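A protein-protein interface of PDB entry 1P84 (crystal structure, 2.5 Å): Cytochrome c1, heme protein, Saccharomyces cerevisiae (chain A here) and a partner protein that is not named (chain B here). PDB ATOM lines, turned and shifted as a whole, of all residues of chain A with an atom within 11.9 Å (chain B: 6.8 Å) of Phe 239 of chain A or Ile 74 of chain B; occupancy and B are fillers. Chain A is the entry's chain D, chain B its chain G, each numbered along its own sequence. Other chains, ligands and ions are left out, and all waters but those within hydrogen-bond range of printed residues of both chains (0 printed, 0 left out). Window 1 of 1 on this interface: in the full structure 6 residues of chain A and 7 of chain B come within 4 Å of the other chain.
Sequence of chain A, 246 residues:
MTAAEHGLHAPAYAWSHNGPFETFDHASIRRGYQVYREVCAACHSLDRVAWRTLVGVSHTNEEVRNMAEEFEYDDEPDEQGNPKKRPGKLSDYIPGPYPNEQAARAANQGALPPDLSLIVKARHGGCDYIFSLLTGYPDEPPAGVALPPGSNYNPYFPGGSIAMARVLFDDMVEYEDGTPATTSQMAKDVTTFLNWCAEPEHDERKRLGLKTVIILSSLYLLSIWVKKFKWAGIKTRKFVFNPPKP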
ATOM      1  N   TRP A 231     -14.602  -2.096  14.817  1.00  0.00           N
ATOM      2  CA  TRP A 231     -13.378  -1.407  15.213  1.00  0.00           C
ATOM      3  C   TRP A 231     -13.160  -1.194  16.729  1.00  0.00           C
ATOM      4  O   TRP A 231     -12.022  -0.960  17.167  1.00  0.00           O
ATOM      5  CB  TRP A 231     -13.291  -0.058  14.489  1.00  0.00           C
ATOM      6  CG  TRP A 231     -12.610  -0.126  13.165  1.00  0.00           C
ATOM      7  CD1 TRP A 231     -13.134  -0.591  11.997  1.00  0.00           C
ATOM      8  CD2 TRP A 231     -11.267   0.274  12.871  1.00  0.00           C
ATOM      9  NE1 TRP A 231     -12.202  -0.508  10.990  1.00  0.00           N
ATOM     10  CE2 TRP A 231     -11.045   0.017  11.498  1.00  0.00           C
ATOM     11  CE3 TRP A 231     -10.224   0.813  13.636  1.00  0.00           C
ATOM     12  CZ2 TRP A 231      -9.818   0.279  10.866  1.00  0.00           C
ATOM     13  CZ3 TRP A 231      -8.996   1.075  13.007  1.00  0.00           C
ATOM     14  CH2 TRP A 231      -8.808   0.804  11.633  1.00  0.00           C
ATOM     15  N   ALA A 232     -14.234  -1.295  17.518  1.00  0.00           N
ATOM     16  CA  ALA A 232     -14.186  -1.086  18.970  1.00  0.00           C
ATOM     17  C   ALA A 232     -13.026  -1.714  19.742  1.00  0.00           C
ATOM     18  O   ALA A 232     -12.543  -1.131  20.711  1.00  0.00           O
ATOM     19  CB  ALA A 232     -15.494  -1.484  19.597  1.00  0.00           C
ATOM     20  N   GLY A 233     -12.578  -2.894  19.336  1.00  0.00           N
ATOM     21  CA  GLY A 233     -11.468  -3.524  20.037  1.00  0.00           C
ATOM     22  C   GLY A 233     -10.142  -2.797  19.860  1.00  0.00           C
ATOM     23  O   GLY A 233      -9.336  -2.700  20.793  1.00  0.00           O
ATOM     24  N   ILE A 234      -9.909  -2.307  18.643  1.00  0.00           N
ATOM     25  CA  ILE A 234      -8.686  -1.578  18.302  1.00  0.00           C
ATOM     26  C   ILE A 234      -8.726  -0.164  18.887  1.00  0.00           C
ATOM     27  O   ILE A 234      -7.757   0.311  19.487  1.00  0.00           O
ATOM     28  CB  ILE A 234      -8.502  -1.511  16.753  1.00  0.00           C
ATOM     29  CG1 ILE A 234      -8.173  -2.904  16.211  1.00  0.00           C
ATOM     30  CG2 ILE A 234      -7.418  -0.508  16.357  1.00  0.00           C
ATOM     31  CD1 ILE A 234      -6.934  -3.539  16.824  1.00  0.00           C
ATOM     32  N   LYS A 235      -9.884   0.472  18.757  1.00  0.00           N
ATOM     33  CA  LYS A 235     -10.080   1.833  19.232  1.00  0.00           C
ATOM     34  C   LYS A 235      -9.827   2.038  20.714  1.00  0.00           C
ATOM     35  O   LYS A 235      -9.161   2.995  21.103  1.00  0.00           O
ATOM     36  CB  LYS A 235     -11.487   2.312  18.878  1.00  0.00           C
ATOM     37  CG  LYS A 235     -11.686   2.623  17.412  1.00  0.00           C
ATOM     38  CD  LYS A 235     -11.403   4.080  17.140  1.00  0.00           C
ATOM     39  CE  LYS A 235     -11.505   4.410  15.651  1.00  0.00           C
ATOM     40  NZ  LYS A 235     -11.198   5.843  15.384  1.00  0.00           N
ATOM     41  N   THR A 236     -10.347   1.140  21.538  1.00  0.00           N
ATOM     42  CA  THR A 236     -10.188   1.261  22.984  1.00  0.00           C
ATOM     43  C   THR A 236      -8.983   0.510  23.544  1.00  0.00           C
ATOM     44  O   THR A 236      -8.781   0.467  24.744  1.00  0.00           O
ATOM     45  CB  THR A 236     -11.482   0.835  23.704  1.00  0.00           C
ATOM     46  OG1 THR A 236     -11.754  -0.546  23.432  1.00  0.00           O
ATOM     47  CG2 THR A 236     -12.658   1.674  23.202  1.00  0.00           C
ATOM     48  N   ARG A 237      -8.170  -0.045  22.656  1.00  0.00           N
ATOM     49  CA  ARG A 237      -6.962  -0.794  23.007  1.00  0.00           C
ATOM     50  C   ARG A 237      -6.027   0.074  23.869  1.00  0.00           C
ATOM     51  O   ARG A 237      -5.932   1.278  23.645  1.00  0.00           O
ATOM     52  CB  ARG A 237      -6.283  -1.233  21.696  1.00  0.00           C
ATOM     53  CG  ARG A 237      -4.971  -1.996  21.802  1.00  0.00           C
ATOM     54  CD  ARG A 237      -4.507  -2.488  20.410  1.00  0.00           C
ATOM     55  NE  ARG A 237      -4.356  -1.397  19.441  1.00  0.00           N
ATOM     56  CZ  ARG A 237      -3.536  -1.428  18.394  1.00  0.00           C
ATOM     57  NH1 ARG A 237      -3.452  -0.386  17.577  1.00  0.00           N
ATOM     58  NH2 ARG A 237      -2.811  -2.506  18.150  1.00  0.00           N
ATOM     59  N   LYS A 238      -5.368  -0.528  24.866  1.00  0.00           N
ATOM     60  CA  LYS A 238      -4.460   0.208  25.762  1.00  0.00           C
ATOM     61  C   LYS A 238      -3.087  -0.431  25.927  1.00  0.00           C
ATOM     62  O   LYS A 238      -2.971  -1.655  26.009  1.00  0.00           O
ATOM     63  CB  LYS A 238      -5.112   0.418  27.138  1.00  0.00           C
ATOM     64  CG  LYS A 238      -6.469   1.110  27.033  1.00  0.00           C
ATOM     65  CD  LYS A 238      -6.988   1.695  28.323  1.00  0.00           C
ATOM     66  CE  LYS A 238      -8.298   2.436  28.043  1.00  0.00           C
ATOM     67  NZ  LYS A 238      -8.871   3.149  29.237  1.00  0.00           N
ATOM     68  N   PHE A 239      -2.054   0.409  25.981  1.00  0.00           N
ATOM     69  CA  PHE A 239      -0.664  -0.041  26.125  1.00  0.00           C
ATOM     70  C   PHE A 239       0.009   0.403  27.442  1.00  0.00           C
ATOM     71  O   PHE A 239      -0.413   1.377  28.071  1.00  0.00           O
ATOM     72  CB  PHE A 239       0.177   0.495  24.960  1.00  0.00           C
ATOM     73  CG  PHE A 239      -0.246  -0.010  23.611  1.00  0.00           C
ATOM     74  CD1 PHE A 239      -1.369   0.506  22.980  1.00  0.00           C
ATOM     75  CD2 PHE A 239       0.483  -1.005  22.966  1.00  0.00           C
ATOM     76  CE1 PHE A 239      -1.769   0.033  21.723  1.00  0.00           C
ATOM     77  CE2 PHE A 239       0.095  -1.486  21.713  1.00  0.00           C
ATOM     78  CZ  PHE A 239      -1.036  -0.963  21.090  1.00  0.00           C
ATOM     79  N   VAL A 240       1.045  -0.331  27.853  1.00  0.00           N
ATOM     80  CA  VAL A 240       1.835  -0.025  29.050  1.00  0.00           C
ATOM     81  C   VAL A 240       3.292  -0.407  28.767  1.00  0.00           C
ATOM     82  O   VAL A 240       3.573  -1.454  28.180  1.00  0.00           O
ATOM     83  CB  VAL A 240       1.359  -0.786  30.318  1.00  0.00           C
ATOM     84  CG1 VAL A 240      -0.064  -0.408  30.674  1.00  0.00           C
ATOM     85  CG2 VAL A 240       1.481  -2.283  30.126  1.00  0.00           C
ATOM     86  N   PHE A 241       4.222   0.461  29.141  1.00  0.00           N
ATOM     87  CA  PHE A 241       5.630   0.174  28.907  1.00  0.00           C
ATOM     88  C   PHE A 241       6.380  -0.041  30.225  1.00  0.00           C
ATOM     89  O   PHE A 241       6.213   0.721  31.182  1.00  0.00           O
ATOM     90  CB  PHE A 241       6.266   1.305  28.090  1.00  0.00           C
ATOM     91  CG  PHE A 241       7.712   1.075  27.734  1.00  0.00           C
ATOM     92  CD1 PHE A 241       8.132  -0.140  27.174  1.00  0.00           C
ATOM     93  CD2 PHE A 241       8.656   2.088  27.920  1.00  0.00           C
ATOM     94  CE1 PHE A 241       9.472  -0.351  26.798  1.00  0.00           C
ATOM     95  CE2 PHE A 241       9.998   1.891  27.548  1.00  0.00           C
ATOM     96  CZ  PHE A 241      10.407   0.665  26.982  1.00  0.00           C
ATOM     97  N   ASN A 242       7.154  -1.122  30.279  1.00  0.00           N
ATOM     98  CA  ASN A 242       7.955  -1.460  31.446  1.00  0.00           C
ATOM     99  C   ASN A 242       9.367  -1.729  30.948  1.00  0.00           C
ATOM    100  O   ASN A 242       9.686  -2.833  30.509  1.00  0.00           O
ATOM    101  CB  ASN A 242       7.388  -2.687  32.160  1.00  0.00           C
ATOM    102  CG  ASN A 242       6.254  -2.336  33.082  1.00  0.00           C
ATOM    103  OD1 ASN A 242       6.422  -1.528  33.988  1.00  0.00           O
ATOM    104  ND2 ASN A 242       5.088  -2.933  32.862  1.00  0.00           N
ATOM    105  N   PRO A 243      10.233  -0.710  31.003  1.00  0.00           N
ATOM    106  CA  PRO A 243      11.621  -0.806  30.557  1.00  0.00           C
ATOM    107  C   PRO A 243      12.345  -2.065  31.024  1.00  0.00           C
ATOM    108  O   PRO A 243      12.496  -2.312  32.222  1.00  0.00           O
ATOM    109  CB  PRO A 243      12.244   0.459  31.129  1.00  0.00           C
ATOM    110  CG  PRO A 243      11.112   1.428  31.079  1.00  0.00           C
ATOM    111  CD  PRO A 243       9.961   0.613  31.588  1.00  0.00           C
ATOM    112  N   LEU B  41       6.083  11.856  20.760  1.00  0.00           N
ATOM    113  CA  LEU B  41       7.246  11.598  19.918  1.00  0.00           C
ATOM    114  C   LEU B  41       8.375  12.604  20.115  1.00  0.00           C
ATOM    115  O   LEU B  41       8.153  13.732  20.561  1.00  0.00           O
ATOM    116  CB  LEU B  41       6.848  11.608  18.435  1.00  0.00           C
ATOM    117  CG  LEU B  41       5.840  10.570  17.951  1.00  0.00           C
ATOM    118  CD1 LEU B  41       5.272  10.987  16.601  1.00  0.00           C
ATOM    119  CD2 LEU B  41       6.497   9.199  17.881  1.00  0.00           C
ATOM    120  N   ARG B  69      12.109   3.748  21.633  1.00  0.00           N
ATOM    121  CA  ARG B  69      11.659   4.310  20.366  1.00  0.00           C
ATOM    122  C   ARG B  69      10.428   3.536  19.911  1.00  0.00           C
ATOM    123  O   ARG B  69       9.430   4.132  19.474  1.00  0.00           O
ATOM    124  CB  ARG B  69      12.743   4.232  19.286  1.00  0.00           C
ATOM    125  CG  ARG B  69      12.425   5.106  18.071  1.00  0.00           C
ATOM    126  CD  ARG B  69      13.407   4.946  16.914  1.00  0.00           C
ATOM    127  NE  ARG B  69      13.212   3.664  16.263  1.00  0.00           N
ATOM    128  CZ  ARG B  69      12.881   3.496  14.990  1.00  0.00           C
ATOM    129  NH1 ARG B  69      12.722   2.266  14.529  1.00  0.00           N
ATOM    130  NH2 ARG B  69      12.733   4.531  14.178  1.00  0.00           N
ATOM    131  N   ALA B  70      10.485   2.212  20.084  1.00  0.00           N
ATOM    132  CA  ALA B  70       9.398   1.323  19.699  1.00  0.00           C
ATOM    133  C   ALA B  70       8.112   1.664  20.434  1.00  0.00           C
ATOM    134  O   ALA B  70       7.047   1.763  19.819  1.00  0.00           O
ATOM    135  CB  ALA B  70       9.783  -0.120  19.961  1.00  0.00           C
ATOM    136  N   TYR B  71       8.213   1.874  21.743  1.00  0.00           N
ATOM    137  CA  TYR B  71       7.029   2.209  22.528  1.00  0.00           C
ATOM    138  C   TYR B  71       6.450   3.559  22.125  1.00  0.00           C
ATOM    139  O   TYR B  71       5.227   3.742  22.098  1.00  0.00           O
ATOM    140  CB  TYR B  71       7.327   2.210  24.037  1.00  0.00           C
ATOM    141  CG  TYR B  71       6.145   2.670  24.875  1.00  0.00           C
ATOM    142  CD1 TYR B  71       4.910   2.032  24.782  1.00  0.00           C
ATOM    143  CD2 TYR B  71       6.250   3.776  25.718  1.00  0.00           C
ATOM    144  CE1 TYR B  71       3.805   2.479  25.503  1.00  0.00           C
ATOM    145  CE2 TYR B  71       5.148   4.237  26.446  1.00  0.00           C
ATOM    146  CZ  TYR B  71       3.929   3.581  26.335  1.00  0.00           C
ATOM    147  OH  TYR B  71       2.846   4.018  27.063  1.00  0.00           O
ATOM    148  N   ARG B  72       7.323   4.513  21.834  1.00  0.00           N
ATOM    149  CA  ARG B  72       6.853   5.833  21.460  1.00  0.00           C
ATOM    150  C   ARG B  72       6.106   5.808  20.138  1.00  0.00           C
ATOM    151  O   ARG B  72       5.021   6.385  20.023  1.00  0.00           O
ATOM    152  CB  ARG B  72       8.004   6.844  21.435  1.00  0.00           C
ATOM    153  CG  ARG B  72       8.522   7.201  22.837  1.00  0.00           C
ATOM    154  CD  ARG B  72       9.371   8.446  22.824  1.00  0.00           C
ATOM    155  NE  ARG B  72      10.541   8.319  21.962  1.00  0.00           N
ATOM    156  CZ  ARG B  72      11.715   7.845  22.359  1.00  0.00           C
ATOM    157  NH1 ARG B  72      12.724   7.774  21.499  1.00  0.00           N
ATOM    158  NH2 ARG B  72      11.881   7.443  23.614  1.00  0.00           N
ATOM    159  N   ILE B  73       6.649   5.079  19.169  1.00  0.00           N
ATOM    160  CA  ILE B  73       6.022   4.982  17.855  1.00  0.00           C
ATOM    161  C   ILE B  73       4.649   4.293  17.884  1.00  0.00           C
ATOM    162  O   ILE B  73       3.686   4.792  17.292  1.00  0.00           O
ATOM    163  CB  ILE B  73       6.978   4.321  16.847  1.00  0.00           C
ATOM    164  CG1 ILE B  73       8.159   5.274  16.588  1.00  0.00           C
ATOM    165  CG2 ILE B  73       6.244   3.967  15.562  1.00  0.00           C
ATOM    166  CD1 ILE B  73       9.286   4.678  15.766  1.00  0.00           C
ATOM    167  N   ILE B  74       4.549   3.183  18.614  1.00  0.00           N
ATOM    168  CA  ILE B  74       3.284   2.460  18.730  1.00  0.00           C
ATOM    169  C   ILE B  74       2.235   3.330  19.423  1.00  0.00           C
ATOM    170  O   ILE B  74       1.090   3.452  18.947  1.00  0.00           O
ATOM    171  CB  ILE B  74       3.458   1.132  19.504  1.00  0.00           C
ATOM    172  CG1 ILE B  74       4.440   0.222  18.764  1.00  0.00           C
ATOM    173  CG2 ILE B  74       2.117   0.423  19.659  1.00  0.00           C
ATOM    174  CD1 ILE B  74       4.772  -1.053  19.499  1.00  0.00           C
ATOM    175  N   ARG B  75       2.645   3.957  20.526  1.00  0.00           N
ATOM    176  CA  ARG B  75       1.779   4.841  21.310  1.00  0.00           C
ATOM    177  C   ARG B  75       1.243   5.985  20.439  1.00  0.00           C
ATOM    178  O   ARG B  75       0.081   6.381  20.555  1.00  0.00           O
ATOM    179  CB  ARG B  75       2.567   5.406  22.496  1.00  0.00           C
ATOM    180  CG  ARG B  75       1.788   6.336  23.432  1.00  0.00           C
ATOM    181  CD  ARG B  75       2.620   7.571  23.766  1.00  0.00           C
ATOM    182  NE  ARG B  75       3.203   7.560  25.102  1.00  0.00           N
ATOM    183  CZ  ARG B  75       4.406   8.047  25.403  1.00  0.00           C
ATOM    184  NH1 ARG B  75       4.834   7.998  26.659  1.00  0.00           N
ATOM    185  NH2 ARG B  75       5.201   8.539  24.460  1.00  0.00           N
ATOM    186  N   ALA B  76       2.089   6.480  19.540  1.00  0.00           N
ATOM    187  CA  ALA B  76       1.712   7.567  18.640  1.00  0.00           C
ATOM    188  C   ALA B  76       0.624   7.137  17.655  1.00  0.00           C
ATOM    189  O   ALA B  76      -0.363   7.852  17.459  1.00  0.00           O
ATOM    190  CB  ALA B  76       2.941   8.075  17.887  1.00  0.00           C
ATOM    191  N   HIS B  77       0.806   5.965  17.043  1.00  0.00           N
ATOM    192  CA  HIS B  77      -0.160   5.437  16.084  1.00  0.00           C
ATOM    193  C   HIS B  77      -1.527   5.214  16.717  1.00  0.00           C
ATOM    194  O   HIS B  77      -2.564   5.507  16.100  1.00  0.00           O
ATOM    195  CB  HIS B  77       0.344   4.127  15.484  1.00  0.00           C
ATOM    196  CG  HIS B  77       1.324   4.307  14.366  1.00  0.00           C
ATOM    197  ND1 HIS B  77       2.637   3.887  14.447  1.00  0.00           N
ATOM    198  CD2 HIS B  77       1.172   4.823  13.123  1.00  0.00           C
ATOM    199  CE1 HIS B  77       3.249   4.132  13.303  1.00  0.00           C
ATOM    200  NE2 HIS B  77       2.382   4.700  12.482  1.00  0.00           N
ATOM    201  N   GLN B  78      -1.529   4.711  17.955  1.00  0.00           N
ATOM    202  CA  GLN B  78      -2.777   4.446  18.668  1.00  0.00           C
ATOM    203  C   GLN B  78      -3.523   5.733  19.000  1.00  0.00           C
ATOM    204  O   GLN B  78      -4.749   5.799  18.863  1.00  0.00           O
ATOM    205  CB  GLN B  78      -2.514   3.644  19.937  1.00  0.00           C
ATOM    206  CG  GLN B  78      -3.763   3.371  20.767  1.00  0.00           C
ATOM    207  CD  GLN B  78      -4.753   2.438  20.094  1.00  0.00           C
ATOM    208  OE1 GLN B  78      -4.369   1.546  19.340  1.00  0.00           O
ATOM    209  NE2 GLN B  78      -6.037   2.627  20.383  1.00  0.00           N
ATOM    210  N   THR B  79      -2.788   6.761  19.422  1.00  0.00           N
ATOM    211  CA  THR B  79      -3.421   8.036  19.750  1.00  0.00           C
ATOM    212  C   THR B  79      -3.981   8.640  18.467  1.00  0.00           C
ATOM    213  O   THR B  79      -5.128   9.081  18.421  1.00  0.00           O
ATOM    214  CB  THR B  79      -2.422   9.036  20.368  1.00  0.00           C
ATOM    215  OG1 THR B  79      -1.531   8.341  21.248  1.00  0.00           O
ATOM    216  CG2 THR B  79      -3.168  10.095  21.160  1.00  0.00           C
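OE1 of Gln 78 of chain B lies within hydrogen-bond range of NH1 of Arg 237 of chain A. The backbone carbonyl oxygen (O) of Ile 234 of chain A lies within hydrogen-bond range of the side-chain amide nitrogen (NE2) of Gln 78 of chain B, 3.0 Å away. The side-chain amide nitrogen of Gln 78 of chain B sits at hydrogen-bond distance from the backbone carbonyl oxygen of Lys 235 of chain A, 3.2 Å away.
Phe 239 of chain A touches Ile 74 of chain B. Gln 78 of chain B touches Phe 239 of chain A (OE1 to CE1, 3.8 Å). Phe 241 of chain A touches Tyr 71 of chain B.
Ala 232 of chain A touches none of the printed residues of chain B. Of the printed residues of chain B, Ile 234 of chain A touches Gln 78. Printed residues of chain B within 4 Å of Lys 235 of chain A: Gln 78. Of the printed residues of chain B, Arg 237 of chain A touches Gln 78 (2.8 Å). Of chain B, only Ile 74 and Gln 78 come within 4 Å of Phe 239 of chain A. Of the printed residues of chain B, Phe 241 of chain A touches Tyr 71 (3.4 Å). Tyr 71 of chain B touches just one residue of chain A: Phe 241 (3.4 Å). No residue of chain A comes within 4 Å of Ile 73 of chain B. Printed residues of chain A within 4 Å of Ile 74 of chain B: Phe 239. No residue of chain A comes within 4 Å of Ala 76 of chain B. Of chain A, only Ile 234, Lys 235, Arg 237 and Phe 239 come within 4 Å of Gln 78 of chain B. Thr 79 of chain B touches none of the printed residues of chain A. The nearest residue of chain A that does not touch Ile 74 of chain B is Arg 237 of chain A (5.9 Å).
Of the 13 printed residues of chain A, 5 touch a printed residue of chain B. Hydrophobic or aromatic side chains of chain A within 4 Å of the printed part of chain B: Phe 239 and Phe 241.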
